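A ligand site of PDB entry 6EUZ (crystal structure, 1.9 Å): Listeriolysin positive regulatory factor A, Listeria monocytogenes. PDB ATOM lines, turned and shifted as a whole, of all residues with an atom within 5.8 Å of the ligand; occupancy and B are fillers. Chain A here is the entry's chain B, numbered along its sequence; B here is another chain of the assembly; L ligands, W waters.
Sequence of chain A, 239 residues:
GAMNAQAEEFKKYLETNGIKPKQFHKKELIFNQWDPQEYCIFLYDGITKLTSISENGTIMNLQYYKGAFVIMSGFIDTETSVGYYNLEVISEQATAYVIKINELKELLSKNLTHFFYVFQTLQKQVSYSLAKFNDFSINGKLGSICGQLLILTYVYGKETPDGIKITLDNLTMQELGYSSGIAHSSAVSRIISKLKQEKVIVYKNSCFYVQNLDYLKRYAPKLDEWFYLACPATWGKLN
A sulfur (S1) of the ligand lies close to the backbone carbonyl oxygen of Ser 179 (3.4 Å).
Merely in contact with the ligand: Leu 62 (3.3 Å), Ser 129 of chain A (3.6 Å), Phe 133 of chain A (3.3 Å), Phe 136 of chain A (3.7 Å), Ser 144 (3.4 Å), Tyr 178 (3.9 Å), Ser 180 (3.4 Å), Ser 129 of chain B (3.4 Å), Lys 132 of chain B (3.8 Å) and Phe 133 of chain B (3.5 Å).
The nearest printed residue that does not touch the ligand is Phe 136 of chain B (4.1 Å).
Water W1 lies within hydrogen-bond range of an oxygen (O2) of the ligand (2.4 Å), the backbone carbonyl oxygen (O) of Ser 179 (2.6 Å), the side-chain amide oxygen (OE1) of Gln 148 (3.2 Å), the side-chain amino group (NZ) of Lys 132 of chain A (3.3 Å) and the side-chain hydroxyl (OH) of Tyr 128 (3.3 Å).
Water W2 lies within hydrogen-bond range of OG of Ser 129 of chain A (2.7 Å) and O4 of the ligand (2.8 Å).
NE2 of Gln 63 sits at hydrogen-bond distance from OG of Ser 129 of chain A.
OH of Tyr 128 lies within hydrogen-bond range of NZ of Lys 132 of chain A (3.1 Å).
The backbone carbonyl oxygen of Ser 179 lies within hydrogen-bond range of the side-chain amino group of Lys 132 of chain A, 3.4 Å away.
OE1 of Gln 148 lies within hydrogen-bond range of NZ of Lys 132 of chain A (2.7 Å).
The side-chain amide oxygen (OE1) of Gln 148 sits close to the backbone carbonyl oxygen (O) of Ser 179 (3.4 Å).
An oxygen (O4) of the ligand lies within hydrogen-bond range of the side-chain amide nitrogen (NE2) of Gln 63 (2.8 Å).
The side-chain hydroxyl of Tyr 128 sits at hydrogen-bond distance from an oxygen (O1) of the ligand.
O1 of the ligand lies within salt-bridge range of NZ of Lys 132 of chain A (2.9 Å).
S1 of the ligand lies close to N of Gly 181.
N of Tyr 64 lies within hydrogen-bond range of O2 of the ligand (3.3 Å).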
ATOM      1  N   ASN A  61      14.084 -24.636  26.331  1.00  0.00           N
ATOM      2  CA  ASN A  61      12.718 -24.904  25.879  1.00  0.00           C
ATOM      3  C   ASN A  61      12.425 -24.015  24.674  1.00  0.00           C
ATOM      4  O   ASN A  61      12.382 -22.782  24.807  1.00  0.00           O
ATOM      5  CB  ASN A  61      11.723 -24.661  27.001  1.00  0.00           C
ATOM      6  CG  ASN A  61      12.055 -25.469  28.234  1.00  0.00           C
ATOM      7  OD1 ASN A  61      12.004 -26.693  28.214  1.00  0.00           O
ATOM      8  ND2 ASN A  61      12.449 -24.796  29.309  1.00  0.00           N
ATOM      9  N   LEU A  62      12.195 -24.639  23.529  1.00  0.00           N
ATOM     10  CA  LEU A  62      12.112 -23.939  22.263  1.00  0.00           C
ATOM     11  C   LEU A  62      10.700 -23.681  21.788  1.00  0.00           C
ATOM     12  O   LEU A  62      10.452 -22.682  21.114  1.00  0.00           O
ATOM     13  CB  LEU A  62      12.849 -24.743  21.184  1.00  0.00           C
ATOM     14  CG  LEU A  62      14.335 -24.997  21.395  1.00  0.00           C
ATOM     15  CD1 LEU A  62      14.830 -25.998  20.376  1.00  0.00           C
ATOM     16  CD2 LEU A  62      15.113 -23.705  21.272  1.00  0.00           C
ATOM     17  N   GLN A  63       9.759 -24.572  22.064  1.00  0.00           N
ATOM     18  CA  GLN A  63       8.441 -24.400  21.470  1.00  0.00           C
ATOM     19  C   GLN A  63       7.495 -25.383  22.144  1.00  0.00           C
ATOM     20  O   GLN A  63       7.923 -26.430  22.624  1.00  0.00           O
ATOM     21  CB  GLN A  63       8.491 -24.641  19.961  1.00  0.00           C
ATOM     22  CG  GLN A  63       7.244 -24.190  19.228  1.00  0.00           C
ATOM     23  CD  GLN A  63       7.562 -23.789  17.820  1.00  0.00           C
ATOM     24  OE1 GLN A  63       7.811 -24.638  16.965  1.00  0.00           O
ATOM     25  NE2 GLN A  63       7.594 -22.480  17.565  1.00  0.00           N
ATOM     26  N   TYR A  64       6.215 -25.012  22.189  1.00  0.00           N
ATOM     27  CA  TYR A  64       5.184 -25.826  22.809  1.00  0.00           C
ATOM     28  C   TYR A  64       4.120 -26.152  21.787  1.00  0.00           C
ATOM     29  O   TYR A  64       3.785 -25.316  20.943  1.00  0.00           O
ATOM     30  CB  TYR A  64       4.570 -25.098  23.987  1.00  0.00           C
ATOM     31  CG  TYR A  64       5.538 -24.933  25.114  1.00  0.00           C
ATOM     32  CD1 TYR A  64       6.585 -24.021  25.024  1.00  0.00           C
ATOM     33  CD2 TYR A  64       5.432 -25.696  26.260  1.00  0.00           C
ATOM     34  CE1 TYR A  64       7.492 -23.879  26.052  1.00  0.00           C
ATOM     35  CE2 TYR A  64       6.338 -25.543  27.306  1.00  0.00           C
ATOM     36  CZ  TYR A  64       7.362 -24.642  27.196  1.00  0.00           C
ATOM     37  OH  TYR A  64       8.256 -24.502  28.228  1.00  0.00           O
ATOM     38  N   TYR A 128       3.320 -18.527  13.190  1.00  0.00           N
ATOM     39  CA  TYR A 128       3.262 -18.400  14.641  1.00  0.00           C
ATOM     40  C   TYR A 128       4.555 -17.782  15.184  1.00  0.00           C
ATOM     41  O   TYR A 128       4.509 -16.835  15.984  1.00  0.00           O
ATOM     42  CB  TYR A 128       3.032 -19.786  15.262  1.00  0.00           C
ATOM     43  CG  TYR A 128       3.122 -19.858  16.777  1.00  0.00           C
ATOM     44  CD1 TYR A 128       2.031 -19.550  17.564  1.00  0.00           C
ATOM     45  CD2 TYR A 128       4.299 -20.238  17.407  1.00  0.00           C
ATOM     46  CE1 TYR A 128       2.109 -19.614  18.959  1.00  0.00           C
ATOM     47  CE2 TYR A 128       4.393 -20.309  18.802  1.00  0.00           C
ATOM     48  CZ  TYR A 128       3.289 -20.001  19.557  1.00  0.00           C
ATOM     49  OH  TYR A 128       3.381 -20.058  20.934  1.00  0.00           O
ATOM     50  N   SER A 129       5.713 -18.313  14.777  1.00  0.00           N
ATOM     51  CA  SER A 129       6.984 -17.794  15.273  1.00  0.00           C
ATOM     52  C   SER A 129       7.209 -16.355  14.823  1.00  0.00           C
ATOM     53  O   SER A 129       7.759 -15.546  15.594  1.00  0.00           O
ATOM     54  CB  SER A 129       8.150 -18.672  14.823  1.00  0.00           C
ATOM     55  OG  SER A 129       8.051 -19.969  15.400  1.00  0.00           O
ATOM     56  N   LEU A 130       6.759 -16.003  13.613  1.00  0.00           N
ATOM     57  CA  LEU A 130       6.928 -14.628  13.156  1.00  0.00           C
ATOM     58  C   LEU A 130       6.064 -13.667  13.967  1.00  0.00           C
ATOM     59  O   LEU A 130       6.500 -12.556  14.276  1.00  0.00           O
ATOM     60  CB  LEU A 130       6.579 -14.507  11.667  1.00  0.00           C
ATOM     61  CG  LEU A 130       7.570 -15.123  10.687  1.00  0.00           C
ATOM     62  CD1 LEU A 130       6.936 -15.169   9.294  1.00  0.00           C
ATOM     63  CD2 LEU A 130       8.860 -14.356  10.647  1.00  0.00           C
ATOM     64  N   LYS A 132       5.032 -14.112  17.158  1.00  0.00           N
ATOM     65  CA  LYS A 132       5.639 -13.968  18.486  1.00  0.00           C
ATOM     66  C   LYS A 132       6.845 -13.034  18.430  1.00  0.00           C
ATOM     67  O   LYS A 132       7.070 -12.244  19.363  1.00  0.00           O
ATOM     68  CB  LYS A 132       6.053 -15.317  19.050  1.00  0.00           C
ATOM     69  CG  LYS A 132       4.899 -16.097  19.684  1.00  0.00           C
ATOM     70  CD  LYS A 132       5.228 -16.523  21.133  1.00  0.00           C
ATOM     71  CE  LYS A 132       3.939 -16.845  21.914  1.00  0.00           C
ATOM     72  NZ  LYS A 132       4.102 -17.869  22.986  1.00  0.00           N
ATOM     73  N   PHE A 133       7.622 -13.104  17.348  1.00  0.00           N
ATOM     74  CA  PHE A 133       8.799 -12.252  17.198  1.00  0.00           C
ATOM     75  C   PHE A 133       8.405 -10.787  17.051  1.00  0.00           C
ATOM     76  O   PHE A 133       8.994  -9.897  17.667  1.00  0.00           O
ATOM     77  CB  PHE A 133       9.618 -12.702  15.994  1.00  0.00           C
ATOM     78  CG  PHE A 133      10.813 -11.808  15.680  1.00  0.00           C
ATOM     79  CD1 PHE A 133      11.906 -11.779  16.505  1.00  0.00           C
ATOM     80  CD2 PHE A 133      10.828 -11.039  14.541  1.00  0.00           C
ATOM     81  CE1 PHE A 133      13.005 -10.975  16.207  1.00  0.00           C
ATOM     82  CE2 PHE A 133      11.907 -10.237  14.232  1.00  0.00           C
ATOM     83  CZ  PHE A 133      12.999 -10.213  15.071  1.00  0.00           C
ATOM     84  N   PHE A 136       7.314  -9.495  20.378  1.00  0.00           N
ATOM     85  CA  PHE A 136       8.450  -9.295  21.271  1.00  0.00           C
ATOM     86  C   PHE A 136       9.277  -8.095  20.846  1.00  0.00           C
ATOM     87  O   PHE A 136       9.826  -7.389  21.693  1.00  0.00           O
ATOM     88  CB  PHE A 136       9.333 -10.542  21.312  1.00  0.00           C
ATOM     89  CG  PHE A 136      10.577 -10.345  22.110  1.00  0.00           C
ATOM     90  CD1 PHE A 136      10.529 -10.379  23.495  1.00  0.00           C
ATOM     91  CD2 PHE A 136      11.768 -10.096  21.495  1.00  0.00           C
ATOM     92  CE1 PHE A 136      11.658 -10.185  24.240  1.00  0.00           C
ATOM     93  CE2 PHE A 136      12.922  -9.904  22.244  1.00  0.00           C
ATOM     94  CZ  PHE A 136      12.855  -9.940  23.618  1.00  0.00           C
ATOM     95  N   SER A 144       5.528 -10.920  25.069  1.00  0.00           N
ATOM     96  CA  SER A 144       5.645 -12.373  25.113  1.00  0.00           C
ATOM     97  C   SER A 144       4.686 -12.965  26.127  1.00  0.00           C
ATOM     98  O   SER A 144       3.959 -13.931  25.839  1.00  0.00           O
ATOM     99  CB  SER A 144       7.076 -12.778  25.437  1.00  0.00           C
ATOM    100  OG  SER A 144       7.988 -12.314  24.469  1.00  0.00           O
ATOM    101  N   GLN A 148       1.288 -15.319  25.529  1.00  0.00           N
ATOM    102  CA  GLN A 148       1.134 -16.648  26.112  1.00  0.00           C
ATOM    103  C   GLN A 148      -0.179 -16.758  26.870  1.00  0.00           C
ATOM    104  O   GLN A 148      -0.951 -17.706  26.681  1.00  0.00           O
ATOM    105  CB  GLN A 148       2.318 -16.937  27.026  1.00  0.00           C
ATOM    106  CG  GLN A 148       2.444 -18.390  27.367  1.00  0.00           C
ATOM    107  CD  GLN A 148       2.350 -19.266  26.130  1.00  0.00           C
ATOM    108  OE1 GLN A 148       2.749 -18.856  25.045  1.00  0.00           O
ATOM    109  NE2 GLN A 148       1.791 -20.458  26.292  1.00  0.00           N
ATOM    110  N   ILE A 151      -2.994 -16.954  24.339  1.00  0.00           N
ATOM    111  CA  ILE A 151      -3.105 -18.336  23.883  1.00  0.00           C
ATOM    112  C   ILE A 151      -3.887 -19.173  24.887  1.00  0.00           C
ATOM    113  O   ILE A 151      -4.874 -19.848  24.555  1.00  0.00           O
ATOM    114  CB  ILE A 151      -1.706 -18.943  23.658  1.00  0.00           C
ATOM    115  CG1 ILE A 151      -1.053 -18.375  22.403  1.00  0.00           C
ATOM    116  CG2 ILE A 151      -1.763 -20.471  23.594  1.00  0.00           C
ATOM    117  CD1 ILE A 151       0.456 -18.538  22.423  1.00  0.00           C
ATOM    118  N   GLY A 177       6.822 -18.854  31.977  1.00  0.00           N
ATOM    119  CA  GLY A 177       7.978 -18.112  31.481  1.00  0.00           C
ATOM    120  C   GLY A 177       8.646 -18.814  30.311  1.00  0.00           C
ATOM    121  O   GLY A 177       8.911 -18.208  29.269  1.00  0.00           O
ATOM    122  N   TYR A 178       8.936 -20.115  30.469  1.00  0.00           N
ATOM    123  CA  TYR A 178       9.566 -20.858  29.378  1.00  0.00           C
ATOM    124  C   TYR A 178       8.720 -20.808  28.117  1.00  0.00           C
ATOM    125  O   TYR A 178       9.247 -20.673  27.006  1.00  0.00           O
ATOM    126  CB  TYR A 178       9.800 -22.325  29.786  1.00  0.00           C
ATOM    127  CG  TYR A 178      10.838 -22.553  30.874  1.00  0.00           C
ATOM    128  CD1 TYR A 178      11.986 -21.764  30.963  1.00  0.00           C
ATOM    129  CD2 TYR A 178      10.675 -23.577  31.795  1.00  0.00           C
ATOM    130  CE1 TYR A 178      12.936 -21.990  31.950  1.00  0.00           C
ATOM    131  CE2 TYR A 178      11.616 -23.813  32.793  1.00  0.00           C
ATOM    132  CZ  TYR A 178      12.740 -23.018  32.866  1.00  0.00           C
ATOM    133  OH  TYR A 178      13.674 -23.239  33.854  1.00  0.00           O
ATOM    134  N   SER A 179       7.387 -20.906  28.263  1.00  0.00           N
ATOM    135  CA  SER A 179       6.503 -20.832  27.106  1.00  0.00           C
ATOM    136  C   SER A 179       6.482 -19.441  26.496  1.00  0.00           C
ATOM    137  O   SER A 179       6.057 -19.303  25.346  1.00  0.00           O
ATOM    138  CB  SER A 179       5.083 -21.256  27.485  1.00  0.00           C
ATOM    139  OG  SER A 179       4.526 -20.379  28.444  1.00  0.00           O
ATOM    140  N   SER A 180       6.939 -18.420  27.229  1.00  0.00           N
ATOM    141  CA  SER A 180       7.029 -17.053  26.730  1.00  0.00           C
ATOM    142  C   SER A 180       8.475 -16.650  26.421  1.00  0.00           C
ATOM    143  O   SER A 180       8.729 -15.472  26.174  1.00  0.00           O
ATOM    144  CB  SER A 180       6.415 -16.070  27.737  1.00  0.00           C
ATOM    145  OG  SER A 180       5.083 -16.456  28.080  1.00  0.00           O
ATOM    146  N   GLY A 181       9.403 -17.603  26.447  1.00  0.00           N
ATOM    147  CA  GLY A 181      10.787 -17.310  26.121  1.00  0.00           C
ATOM    148  C   GLY A 181      11.563 -16.561  27.192  1.00  0.00           C
ATOM    149  O   GLY A 181      12.606 -15.982  26.888  1.00  0.00           O
ATOM    150  N   ILE A 182      11.087 -16.572  28.431  1.00  0.00           N
ATOM    151  CA  ILE A 182      11.746 -15.893  29.546  1.00  0.00           C
ATOM    152  C   ILE A 182      12.159 -16.952  30.557  1.00  0.00           C
ATOM    153  O   ILE A 182      11.314 -17.693  31.074  1.00  0.00           O
ATOM    154  CB  ILE A 182      10.831 -14.827  30.177  1.00  0.00           C
ATOM    155  CG1 ILE A 182      10.458 -13.769  29.117  1.00  0.00           C
ATOM    156  CG2 ILE A 182      11.504 -14.179  31.374  1.00  0.00           C
ATOM    157  CD1 ILE A 182       9.148 -13.045  29.372  1.00  0.00           C
ATOM    158  N   SER B 129      13.890 -20.460  12.211  1.00  0.00           N
ATOM    159  CA  SER B 129      13.403 -19.605  13.292  1.00  0.00           C
ATOM    160  C   SER B 129      13.712 -20.191  14.657  1.00  0.00           C
ATOM    161  O   SER B 129      13.948 -19.454  15.616  1.00  0.00           O
ATOM    162  CB  SER B 129      11.901 -19.364  13.150  1.00  0.00           C
ATOM    163  OG  SER B 129      11.636 -18.628  11.959  1.00  0.00           O
ATOM    164  N   LEU B 130      13.672 -21.510  14.778  1.00  0.00           N
ATOM    165  CA  LEU B 130      13.972 -22.114  16.059  1.00  0.00           C
ATOM    166  C   LEU B 130      15.434 -21.896  16.428  1.00  0.00           C
ATOM    167  O   LEU B 130      15.759 -21.635  17.585  1.00  0.00           O
ATOM    168  CB  LEU B 130      13.654 -23.614  16.029  1.00  0.00           C
ATOM    169  CG  LEU B 130      12.159 -23.958  15.982  1.00  0.00           C
ATOM    170  CD1 LEU B 130      11.972 -25.439  15.716  1.00  0.00           C
ATOM    171  CD2 LEU B 130      11.459 -23.524  17.262  1.00  0.00           C
ATOM    172  N   LYS B 132      17.490 -19.445  15.377  1.00  0.00           N
ATOM    173  CA  LYS B 132      17.657 -18.039  15.697  1.00  0.00           C
ATOM    174  C   LYS B 132      17.187 -17.739  17.112  1.00  0.00           C
ATOM    175  O   LYS B 132      17.864 -17.034  17.875  1.00  0.00           O
ATOM    176  CB  LYS B 132      16.836 -17.187  14.713  1.00  0.00           C
ATOM    177  CG  LYS B 132      17.563 -16.635  13.484  1.00  0.00           C
ATOM    178  CD  LYS B 132      16.654 -15.586  12.799  1.00  0.00           C
ATOM    179  CE  LYS B 132      17.421 -14.471  12.093  1.00  0.00           C
ATOM    180  NZ  LYS B 132      16.479 -13.536  11.384  1.00  0.00           N
ATOM    181  N   PHE B 133      16.005 -18.218  17.468  1.00  0.00           N
ATOM    182  CA  PHE B 133      15.490 -18.049  18.821  1.00  0.00           C
ATOM    183  C   PHE B 133      16.439 -18.636  19.850  1.00  0.00           C
ATOM    184  O   PHE B 133      16.708 -18.014  20.884  1.00  0.00           O
ATOM    185  CB  PHE B 133      14.118 -18.698  18.926  1.00  0.00           C
ATOM    186  CG  PHE B 133      13.555 -18.705  20.308  1.00  0.00           C
ATOM    187  CD1 PHE B 133      13.011 -17.552  20.840  1.00  0.00           C
ATOM    188  CD2 PHE B 133      13.593 -19.854  21.077  1.00  0.00           C
ATOM    189  CE1 PHE B 133      12.474 -17.547  22.123  1.00  0.00           C
ATOM    190  CE2 PHE B 133      13.064 -19.844  22.363  1.00  0.00           C
ATOM    191  CZ  PHE B 133      12.509 -18.688  22.887  1.00  0.00           C
ATOM    192  N   PHE B 136      19.397 -16.288  20.100  1.00  0.00           N
ATOM    193  CA  PHE B 136      19.015 -15.082  20.814  1.00  0.00           C
ATOM    194  C   PHE B 136      18.827 -15.360  22.297  1.00  0.00           C
ATOM    195  O   PHE B 136      19.285 -14.587  23.151  1.00  0.00           O
ATOM    196  CB  PHE B 136      17.730 -14.488  20.258  1.00  0.00           C
ATOM    197  CG  PHE B 136      17.267 -13.285  21.000  1.00  0.00           C
ATOM    198  CD1 PHE B 136      17.810 -12.044  20.725  1.00  0.00           C
ATOM    199  CD2 PHE B 136      16.331 -13.396  22.013  1.00  0.00           C
ATOM    200  CE1 PHE B 136      17.402 -10.918  21.406  1.00  0.00           C
ATOM    201  CE2 PHE B 136      15.922 -12.275  22.708  1.00  0.00           C
ATOM    202  CZ  PHE B 136      16.472 -11.032  22.411  1.00  0.00           C
HETATM  203  C1  LIG L   1       9.080 -16.687  19.788  1.00  0.00           C
HETATM  204  O1  LIG L   1       6.072 -19.567  21.649  1.00  0.00           O
HETATM  205  C2  LIG L   1       6.706 -20.632  21.804  1.00  0.00           C
HETATM  206  O2  LIG L   1       6.210 -21.758  21.952  1.00  0.00           O
HETATM  207  C3  LIG L   1       8.224 -20.419  21.805  1.00  0.00           C
HETATM  208  C4  LIG L   1       8.732 -20.216  23.212  1.00  0.00           C
HETATM  209  S1  LIG L   1       8.788 -18.435  23.506  1.00  0.00           S
HETATM  210  C5  LIG L   1       8.832 -18.095  21.794  1.00  0.00           C
HETATM  211  C6  LIG L   1       9.047 -16.849  21.219  1.00  0.00           C
HETATM  212  O3  LIG L   1       9.255 -15.737  21.980  1.00  0.00           O
HETATM  213  C7  LIG L   1       8.174 -15.300  22.868  1.00  0.00           C
HETATM  214  C8  LIG L   1       9.309 -15.321  19.137  1.00  0.00           C
HETATM  215  C9  LIG L   1      10.709 -14.846  19.116  1.00  0.00           C
HETATM  216  C10 LIG L   1      11.115 -13.946  20.110  1.00  0.00           C
HETATM  217  C11 LIG L   1      12.418 -13.440  20.142  1.00  0.00           C
HETATM  218  C12 LIG L   1      13.346 -13.835  19.198  1.00  0.00           C
HETATM  219  C13 LIG L   1      12.960 -14.748  18.172  1.00  0.00           C
HETATM  220  C14 LIG L   1      13.899 -15.145  17.199  1.00  0.00           C
HETATM  221  C15 LIG L   1      13.552 -16.021  16.206  1.00  0.00           C
HETATM  222  C16 LIG L   1      12.259 -16.517  16.163  1.00  0.00           C
HETATM  223  C17 LIG L   1      11.314 -16.148  17.095  1.00  0.00           C
HETATM  224  C18 LIG L   1      11.633 -15.236  18.144  1.00  0.00           C
HETATM  225  C19 LIG L   1       8.868 -17.830  19.060  1.00  0.00           C
HETATM  226  C20 LIG L   1       8.634 -19.156  19.620  1.00  0.00           C
HETATM  227  O4  LIG L   1       8.445 -20.158  18.924  1.00  0.00           O
HETATM  228  N1  LIG L   1       8.635 -19.243  21.028  1.00  0.00           N
HETATM  229  O   HOH W   1       4.801 -21.021  23.802  1.00  0.00           O
HETATM  230  O   HOH W   2      10.322 -19.856  16.883  1.00  0.00           O
